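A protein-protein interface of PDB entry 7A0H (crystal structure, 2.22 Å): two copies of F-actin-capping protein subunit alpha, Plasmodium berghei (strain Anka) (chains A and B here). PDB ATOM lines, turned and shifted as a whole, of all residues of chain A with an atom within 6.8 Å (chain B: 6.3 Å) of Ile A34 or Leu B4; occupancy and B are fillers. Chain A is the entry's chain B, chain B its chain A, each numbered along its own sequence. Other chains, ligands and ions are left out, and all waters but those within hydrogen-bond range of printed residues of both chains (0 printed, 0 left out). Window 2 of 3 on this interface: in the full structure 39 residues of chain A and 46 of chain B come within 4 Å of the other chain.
The side-chain amide oxygen (OD1) of Asn A30 lies close to the backbone carbonyl oxygen (O) of Glu B7.
The side-chain hydroxyl (OG1) of Thr A33 sits at hydrogen-bond distance from the backbone carbonyl oxygen (O) of Asn A30 (2.5 Å).
Asn A30 touches Phe B11 (OD1 to CB, 3.1 Å). Phe B11 touches Leu A31 (CZ to CD2, 3.7 Å). Ile A34 touches Leu B4. CD1 of Ile A34 touches O of Glu B7 (3.4 Å). Ile A34 touches Lys B8 (CD1 to CA, 3.7 Å).
Ile A34 touches just these residues of chain B: Leu B4, Glu B7 and Lys B8. Leu B4 touches one residue of chain A. Of the printed residues of chain B, Leu A31 touches Phe B11 (3.7 Å). Printed residues of chain B within 4 Å of Asn A30: Glu B7 (3.4 Å) and Phe B11 (3.1 Å). Ser A37 touches none of the printed residues of chain B. Ile A28 touches none of the printed residues of chain B.
Of the 12 printed residues of chain A, 3 touch a printed residue of chain B. Hydrophobic or aromatic side chains of chain A that line the printed part of chain B: Leu A31 and Ile A34. Of the 10 printed residues of chain B, 4 touch a printed residue of chain A. Hydrophobic or aromatic side chains of chain B within 4 Å of the printed part of chain A: Leu B4 and Phe B11. Among the printed residues, 6 pairs touch across the chains. Among the printed residues, no Asp or Glu carboxylate lies within 4 Å of a Lys or Arg side-chain nitrogen of the other chain.
1 position is printed for both chains. Of the 6 pairs that touch across the chains among the printed residues, none has its exchanged pair printed and touching as well.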
ATOM      1  N   LEU A  27     -11.257   3.388   2.487  1.00  0.00           N
ATOM      2  CA  LEU A  27     -11.437   3.190   3.921  1.00  0.00           C
ATOM      3  C   LEU A  27     -12.470   4.137   4.502  1.00  0.00           C
ATOM      4  O   LEU A  27     -13.353   3.724   5.262  1.00  0.00           O
ATOM      5  CB  LEU A  27     -10.117   3.384   4.646  1.00  0.00           C
ATOM      6  CG  LEU A  27      -9.020   2.479   4.131  1.00  0.00           C
ATOM      7  CD1 LEU A  27      -7.810   2.705   4.988  1.00  0.00           C
ATOM      8  CD2 LEU A  27      -9.484   1.058   4.170  1.00  0.00           C
ATOM      9  N   ILE A  28     -12.362   5.418   4.161  1.00  0.00           N
ATOM     10  CA  ILE A  28     -13.279   6.417   4.693  1.00  0.00           C
ATOM     11  C   ILE A  28     -14.708   6.081   4.306  1.00  0.00           C
ATOM     12  O   ILE A  28     -15.623   6.145   5.130  1.00  0.00           O
ATOM     13  CB  ILE A  28     -12.870   7.807   4.210  1.00  0.00           C
ATOM     14  CG1 ILE A  28     -11.462   8.117   4.698  1.00  0.00           C
ATOM     15  CG2 ILE A  28     -13.844   8.829   4.741  1.00  0.00           C
ATOM     16  CD1 ILE A  28     -11.252   7.759   6.133  1.00  0.00           C
ATOM     17  N   SER A  29     -14.921   5.746   3.036  1.00  0.00           N
ATOM     18  CA  SER A  29     -16.245   5.348   2.582  1.00  0.00           C
ATOM     19  C   SER A  29     -16.908   4.419   3.587  1.00  0.00           C
ATOM     20  O   SER A  29     -18.079   4.595   3.945  1.00  0.00           O
ATOM     21  CB  SER A  29     -16.118   4.646   1.225  1.00  0.00           C
ATOM     22  OG  SER A  29     -17.326   4.005   0.852  1.00  0.00           O
ATOM     23  N   ASN A  30     -16.153   3.421   4.056  1.00  0.00           N
ATOM     24  CA  ASN A  30     -16.665   2.457   5.023  1.00  0.00           C
ATOM     25  C   ASN A  30     -16.676   2.995   6.455  1.00  0.00           C
ATOM     26  O   ASN A  30     -17.517   2.568   7.248  1.00  0.00           O
ATOM     27  CB  ASN A  30     -15.860   1.158   4.932  1.00  0.00           C
ATOM     28  CG  ASN A  30     -16.684  -0.069   5.309  1.00  0.00           C
ATOM     29  OD1 ASN A  30     -16.211  -0.935   6.026  1.00  0.00           O
ATOM     30  ND2 ASN A  30     -17.923  -0.134   4.834  1.00  0.00           N
ATOM     31  N   LEU A  31     -15.800   3.942   6.805  1.00  0.00           N
ATOM     32  CA  LEU A  31     -15.726   4.396   8.195  1.00  0.00           C
ATOM     33  C   LEU A  31     -17.003   5.086   8.656  1.00  0.00           C
ATOM     34  O   LEU A  31     -17.385   4.969   9.826  1.00  0.00           O
ATOM     35  CB  LEU A  31     -14.544   5.343   8.382  1.00  0.00           C
ATOM     36  CG  LEU A  31     -13.164   4.702   8.475  1.00  0.00           C
ATOM     37  CD1 LEU A  31     -12.103   5.782   8.577  1.00  0.00           C
ATOM     38  CD2 LEU A  31     -13.133   3.786   9.684  1.00  0.00           C
ATOM     39  N   LYS A  32     -17.654   5.847   7.779  1.00  0.00           N
ATOM     40  CA  LYS A  32     -18.939   6.423   8.159  1.00  0.00           C
ATOM     41  C   LYS A  32     -19.976   5.325   8.337  1.00  0.00           C
ATOM     42  O   LYS A  32     -20.690   5.290   9.346  1.00  0.00           O
ATOM     43  CB  LYS A  32     -19.424   7.439   7.128  1.00  0.00           C
ATOM     44  CG  LYS A  32     -18.785   8.807   7.259  1.00  0.00           C
ATOM     45  CD  LYS A  32     -19.468   9.828   6.357  1.00  0.00           C
ATOM     46  CE  LYS A  32     -20.705  10.440   6.984  1.00  0.00           C
ATOM     47  NZ  LYS A  32     -20.350  11.569   7.896  1.00  0.00           N
ATOM     48  N   THR A  33     -20.069   4.414   7.360  1.00  0.00           N
ATOM     49  CA  THR A  33     -20.991   3.291   7.484  1.00  0.00           C
ATOM     50  C   THR A  33     -20.732   2.541   8.789  1.00  0.00           C
ATOM     51  O   THR A  33     -21.672   2.032   9.410  1.00  0.00           O
ATOM     52  CB  THR A  33     -20.888   2.351   6.270  1.00  0.00           C
ATOM     53  OG1 THR A  33     -19.648   1.634   6.291  1.00  0.00           O
ATOM     54  CG2 THR A  33     -21.016   3.136   4.948  1.00  0.00           C
ATOM     55  N   ILE A  34     -19.471   2.492   9.236  1.00  0.00           N
ATOM     56  CA  ILE A  34     -19.157   1.815  10.491  1.00  0.00           C
ATOM     57  C   ILE A  34     -19.742   2.589  11.668  1.00  0.00           C
ATOM     58  O   ILE A  34     -20.430   2.023  12.526  1.00  0.00           O
ATOM     59  CB  ILE A  34     -17.634   1.622  10.643  1.00  0.00           C
ATOM     60  CG1 ILE A  34     -17.058   0.710   9.554  1.00  0.00           C
ATOM     61  CG2 ILE A  34     -17.299   1.048  11.998  1.00  0.00           C
ATOM     62  CD1 ILE A  34     -17.728  -0.635   9.450  1.00  0.00           C
ATOM     63  N   PHE A  35     -19.523   3.893  11.702  1.00  0.00           N
ATOM     64  CA  PHE A  35     -19.923   4.721  12.829  1.00  0.00           C
ATOM     65  C   PHE A  35     -21.123   5.612  12.530  1.00  0.00           C
ATOM     66  O   PHE A  35     -21.170   6.762  12.964  1.00  0.00           O
ATOM     67  CB  PHE A  35     -18.789   5.620  13.297  1.00  0.00           C
ATOM     68  CG  PHE A  35     -17.580   4.904  13.726  1.00  0.00           C
ATOM     69  CD1 PHE A  35     -17.402   4.618  15.064  1.00  0.00           C
ATOM     70  CD2 PHE A  35     -16.590   4.577  12.819  1.00  0.00           C
ATOM     71  CE1 PHE A  35     -16.277   3.987  15.489  1.00  0.00           C
ATOM     72  CE2 PHE A  35     -15.463   3.939  13.236  1.00  0.00           C
ATOM     73  CZ  PHE A  35     -15.299   3.646  14.575  1.00  0.00           C
ATOM     74  N   GLY A  36     -22.093   5.117  11.765  1.00  0.00           N
ATOM     75  CA  GLY A  36     -23.105   6.014  11.237  1.00  0.00           C
ATOM     76  C   GLY A  36     -24.025   6.624  12.279  1.00  0.00           C
ATOM     77  O   GLY A  36     -24.535   7.733  12.077  1.00  0.00           O
ATOM     78  N   SER A  37     -24.239   5.944  13.412  1.00  0.00           N
ATOM     79  CA  SER A  37     -25.133   6.507  14.423  1.00  0.00           C
ATOM     80  C   SER A  37     -24.464   7.558  15.300  1.00  0.00           C
ATOM     81  O   SER A  37     -25.171   8.291  16.001  1.00  0.00           O
ATOM     82  CB  SER A  37     -25.718   5.405  15.320  1.00  0.00           C
ATOM     83  OG  SER A  37     -24.786   4.983  16.295  1.00  0.00           O
ATOM     84  N   ILE A  41     -18.659  11.678  16.061  1.00  0.00           N
ATOM     85  CA  ILE A  41     -17.535  11.310  15.210  1.00  0.00           C
ATOM     86  C   ILE A  41     -17.857  11.514  13.728  1.00  0.00           C
ATOM     87  O   ILE A  41     -16.934  11.563  12.905  1.00  0.00           O
ATOM     88  CB  ILE A  41     -17.073   9.857  15.441  1.00  0.00           C
ATOM     89  CG1 ILE A  41     -18.164   8.859  15.055  1.00  0.00           C
ATOM     90  CG2 ILE A  41     -16.643   9.617  16.891  1.00  0.00           C
ATOM     91  CD1 ILE A  41     -18.106   8.467  13.616  1.00  0.00           C
ATOM     92  N   ASP B   2     -25.310  -8.458  12.410  1.00  0.00           N
ATOM     93  CA  ASP B   2     -26.322  -7.730  11.652  1.00  0.00           C
ATOM     94  C   ASP B   2     -25.701  -7.122  10.369  1.00  0.00           C
ATOM     95  O   ASP B   2     -24.678  -7.612   9.870  1.00  0.00           O
ATOM     96  CB  ASP B   2     -26.999  -6.671  12.558  1.00  0.00           C
ATOM     97  CG  ASP B   2     -26.039  -5.997  13.545  1.00  0.00           C
ATOM     98  OD1 ASP B   2     -24.857  -5.808  13.205  1.00  0.00           O
ATOM     99  OD2 ASP B   2     -26.482  -5.646  14.665  1.00  0.00           O
ATOM    100  N   SER B   3     -26.357  -6.101   9.807  1.00  0.00           N
ATOM    101  CA  SER B   3     -25.819  -5.415   8.636  1.00  0.00           C
ATOM    102  C   SER B   3     -24.483  -4.773   8.968  1.00  0.00           C
ATOM    103  O   SER B   3     -23.523  -4.869   8.189  1.00  0.00           O
ATOM    104  CB  SER B   3     -26.817  -4.362   8.127  1.00  0.00           C
ATOM    105  OG  SER B   3     -27.287  -3.479   9.146  1.00  0.00           O
ATOM    106  N   LEU B   4     -24.406  -4.125  10.139  1.00  0.00           N
ATOM    107  CA  LEU B   4     -23.149  -3.553  10.602  1.00  0.00           C
ATOM    108  C   LEU B   4     -22.113  -4.632  10.897  1.00  0.00           C
ATOM    109  O   LEU B   4     -20.949  -4.485  10.521  1.00  0.00           O
ATOM    110  CB  LEU B   4     -23.370  -2.679  11.837  1.00  0.00           C
ATOM    111  CG  LEU B   4     -23.850  -1.261  11.523  1.00  0.00           C
ATOM    112  CD1 LEU B   4     -25.321  -1.249  11.086  1.00  0.00           C
ATOM    113  CD2 LEU B   4     -23.599  -0.306  12.686  1.00  0.00           C
ATOM    114  N   LEU B   5     -22.509  -5.721  11.560  1.00  0.00           N
ATOM    115  CA  LEU B   5     -21.534  -6.768  11.834  1.00  0.00           C
ATOM    116  C   LEU B   5     -20.829  -7.199  10.561  1.00  0.00           C
ATOM    117  O   LEU B   5     -19.609  -7.342  10.541  1.00  0.00           O
ATOM    118  CB  LEU B   5     -22.211  -7.991  12.469  1.00  0.00           C
ATOM    119  CG  LEU B   5     -21.349  -9.257  12.592  1.00  0.00           C
ATOM    120  CD1 LEU B   5     -20.436  -9.157  13.814  1.00  0.00           C
ATOM    121  CD2 LEU B   5     -22.179 -10.537  12.643  1.00  0.00           C
ATOM    122  N   ASN B   6     -21.556  -7.295   9.459  1.00  0.00           N
ATOM    123  CA  ASN B   6     -20.906  -7.660   8.210  1.00  0.00           C
ATOM    124  C   ASN B   6     -20.078  -6.512   7.665  1.00  0.00           C
ATOM    125  O   ASN B   6     -19.011  -6.741   7.093  1.00  0.00           O
ATOM    126  CB  ASN B   6     -21.963  -8.155   7.237  1.00  0.00           C
ATOM    127  CG  ASN B   6     -22.706  -9.375   7.774  1.00  0.00           C
ATOM    128  OD1 ASN B   6     -22.089 -10.293   8.338  1.00  0.00           O
ATOM    129  ND2 ASN B   6     -24.029  -9.376   7.637  1.00  0.00           N
ATOM    130  N   GLU B   7     -20.516  -5.273   7.855  1.00  0.00           N
ATOM    131  CA  GLU B   7     -19.697  -4.164   7.378  1.00  0.00           C
ATOM    132  C   GLU B   7     -18.456  -3.970   8.248  1.00  0.00           C
ATOM    133  O   GLU B   7     -17.413  -3.557   7.731  1.00  0.00           O
ATOM    134  CB  GLU B   7     -20.543  -2.878   7.289  1.00  0.00           C
ATOM    135  CG  GLU B   7     -21.724  -2.952   6.281  1.00  0.00           C
ATOM    136  CD  GLU B   7     -21.287  -3.237   4.833  1.00  0.00           C
ATOM    137  OE1 GLU B   7     -20.369  -2.557   4.320  1.00  0.00           O
ATOM    138  OE2 GLU B   7     -21.863  -4.155   4.205  1.00  0.00           O
ATOM    139  N   LYS B   8     -18.547  -4.255   9.557  1.00  0.00           N
ATOM    140  CA  LYS B   8     -17.365  -4.190  10.413  1.00  0.00           C
ATOM    141  C   LYS B   8     -16.344  -5.248  10.008  1.00  0.00           C
ATOM    142  O   LYS B   8     -15.132  -5.059  10.189  1.00  0.00           O
ATOM    143  CB  LYS B   8     -17.726  -4.401  11.891  1.00  0.00           C
ATOM    144  CG  LYS B   8     -18.660  -3.372  12.568  1.00  0.00           C
ATOM    145  CD  LYS B   8     -18.924  -3.706  14.076  1.00  0.00           C
ATOM    146  CE  LYS B   8     -19.892  -2.734  14.795  1.00  0.00           C
ATOM    147  NZ  LYS B   8     -20.093  -3.077  16.242  1.00  0.00           N
ATOM    148  N   LYS B   9     -16.832  -6.369   9.471  1.00  0.00           N
ATOM    149  CA  LYS B   9     -15.994  -7.474   9.040  1.00  0.00           C
ATOM    150  C   LYS B   9     -15.324  -7.116   7.736  1.00  0.00           C
ATOM    151  O   LYS B   9     -14.131  -7.400   7.532  1.00  0.00           O
ATOM    152  CB  LYS B   9     -16.844  -8.729   8.867  1.00  0.00           C
ATOM    153  CG  LYS B   9     -17.323  -9.360  10.167  1.00  0.00           C
ATOM    154  CD  LYS B   9     -17.918 -10.745   9.931  1.00  0.00           C
ATOM    155  CE  LYS B   9     -18.312 -11.407  11.240  1.00  0.00           C
ATOM    156  NZ  LYS B   9     -18.827 -12.774  11.021  1.00  0.00           N
ATOM    157  N   PHE B  11     -14.573  -4.287   6.807  1.00  0.00           N
ATOM    158  CA  PHE B  11     -13.541  -3.297   7.069  1.00  0.00           C
ATOM    159  C   PHE B  11     -12.323  -3.915   7.740  1.00  0.00           C
ATOM    160  O   PHE B  11     -11.190  -3.611   7.355  1.00  0.00           O
ATOM    161  CB  PHE B  11     -14.117  -2.192   7.955  1.00  0.00           C
ATOM    162  CG  PHE B  11     -13.115  -1.188   8.386  1.00  0.00           C
ATOM    163  CD1 PHE B  11     -12.607  -0.281   7.490  1.00  0.00           C
ATOM    164  CD2 PHE B  11     -12.689  -1.138   9.687  1.00  0.00           C
ATOM    165  CE1 PHE B  11     -11.690   0.636   7.892  1.00  0.00           C
ATOM    166  CE2 PHE B  11     -11.771  -0.224  10.083  1.00  0.00           C
ATOM    167  CZ  PHE B  11     -11.271   0.664   9.191  1.00  0.00           C
ATOM    168  N   PHE B  35     -13.264  -2.551  18.975  1.00  0.00           N
ATOM    169  CA  PHE B  35     -14.299  -3.565  18.895  1.00  0.00           C
ATOM    170  C   PHE B  35     -14.099  -4.721  19.867  1.00  0.00           C
ATOM    171  O   PHE B  35     -14.727  -5.760  19.680  1.00  0.00           O
ATOM    172  CB  PHE B  35     -14.368  -4.145  17.483  1.00  0.00           C
ATOM    173  CG  PHE B  35     -14.468  -3.126  16.390  1.00  0.00           C
ATOM    174  CD1 PHE B  35     -15.687  -2.707  15.917  1.00  0.00           C
ATOM    175  CD2 PHE B  35     -13.319  -2.620  15.802  1.00  0.00           C
ATOM    176  CE1 PHE B  35     -15.760  -1.804  14.903  1.00  0.00           C
ATOM    177  CE2 PHE B  35     -13.400  -1.711  14.791  1.00  0.00           C
ATOM    178  CZ  PHE B  35     -14.620  -1.303  14.346  1.00  0.00           C
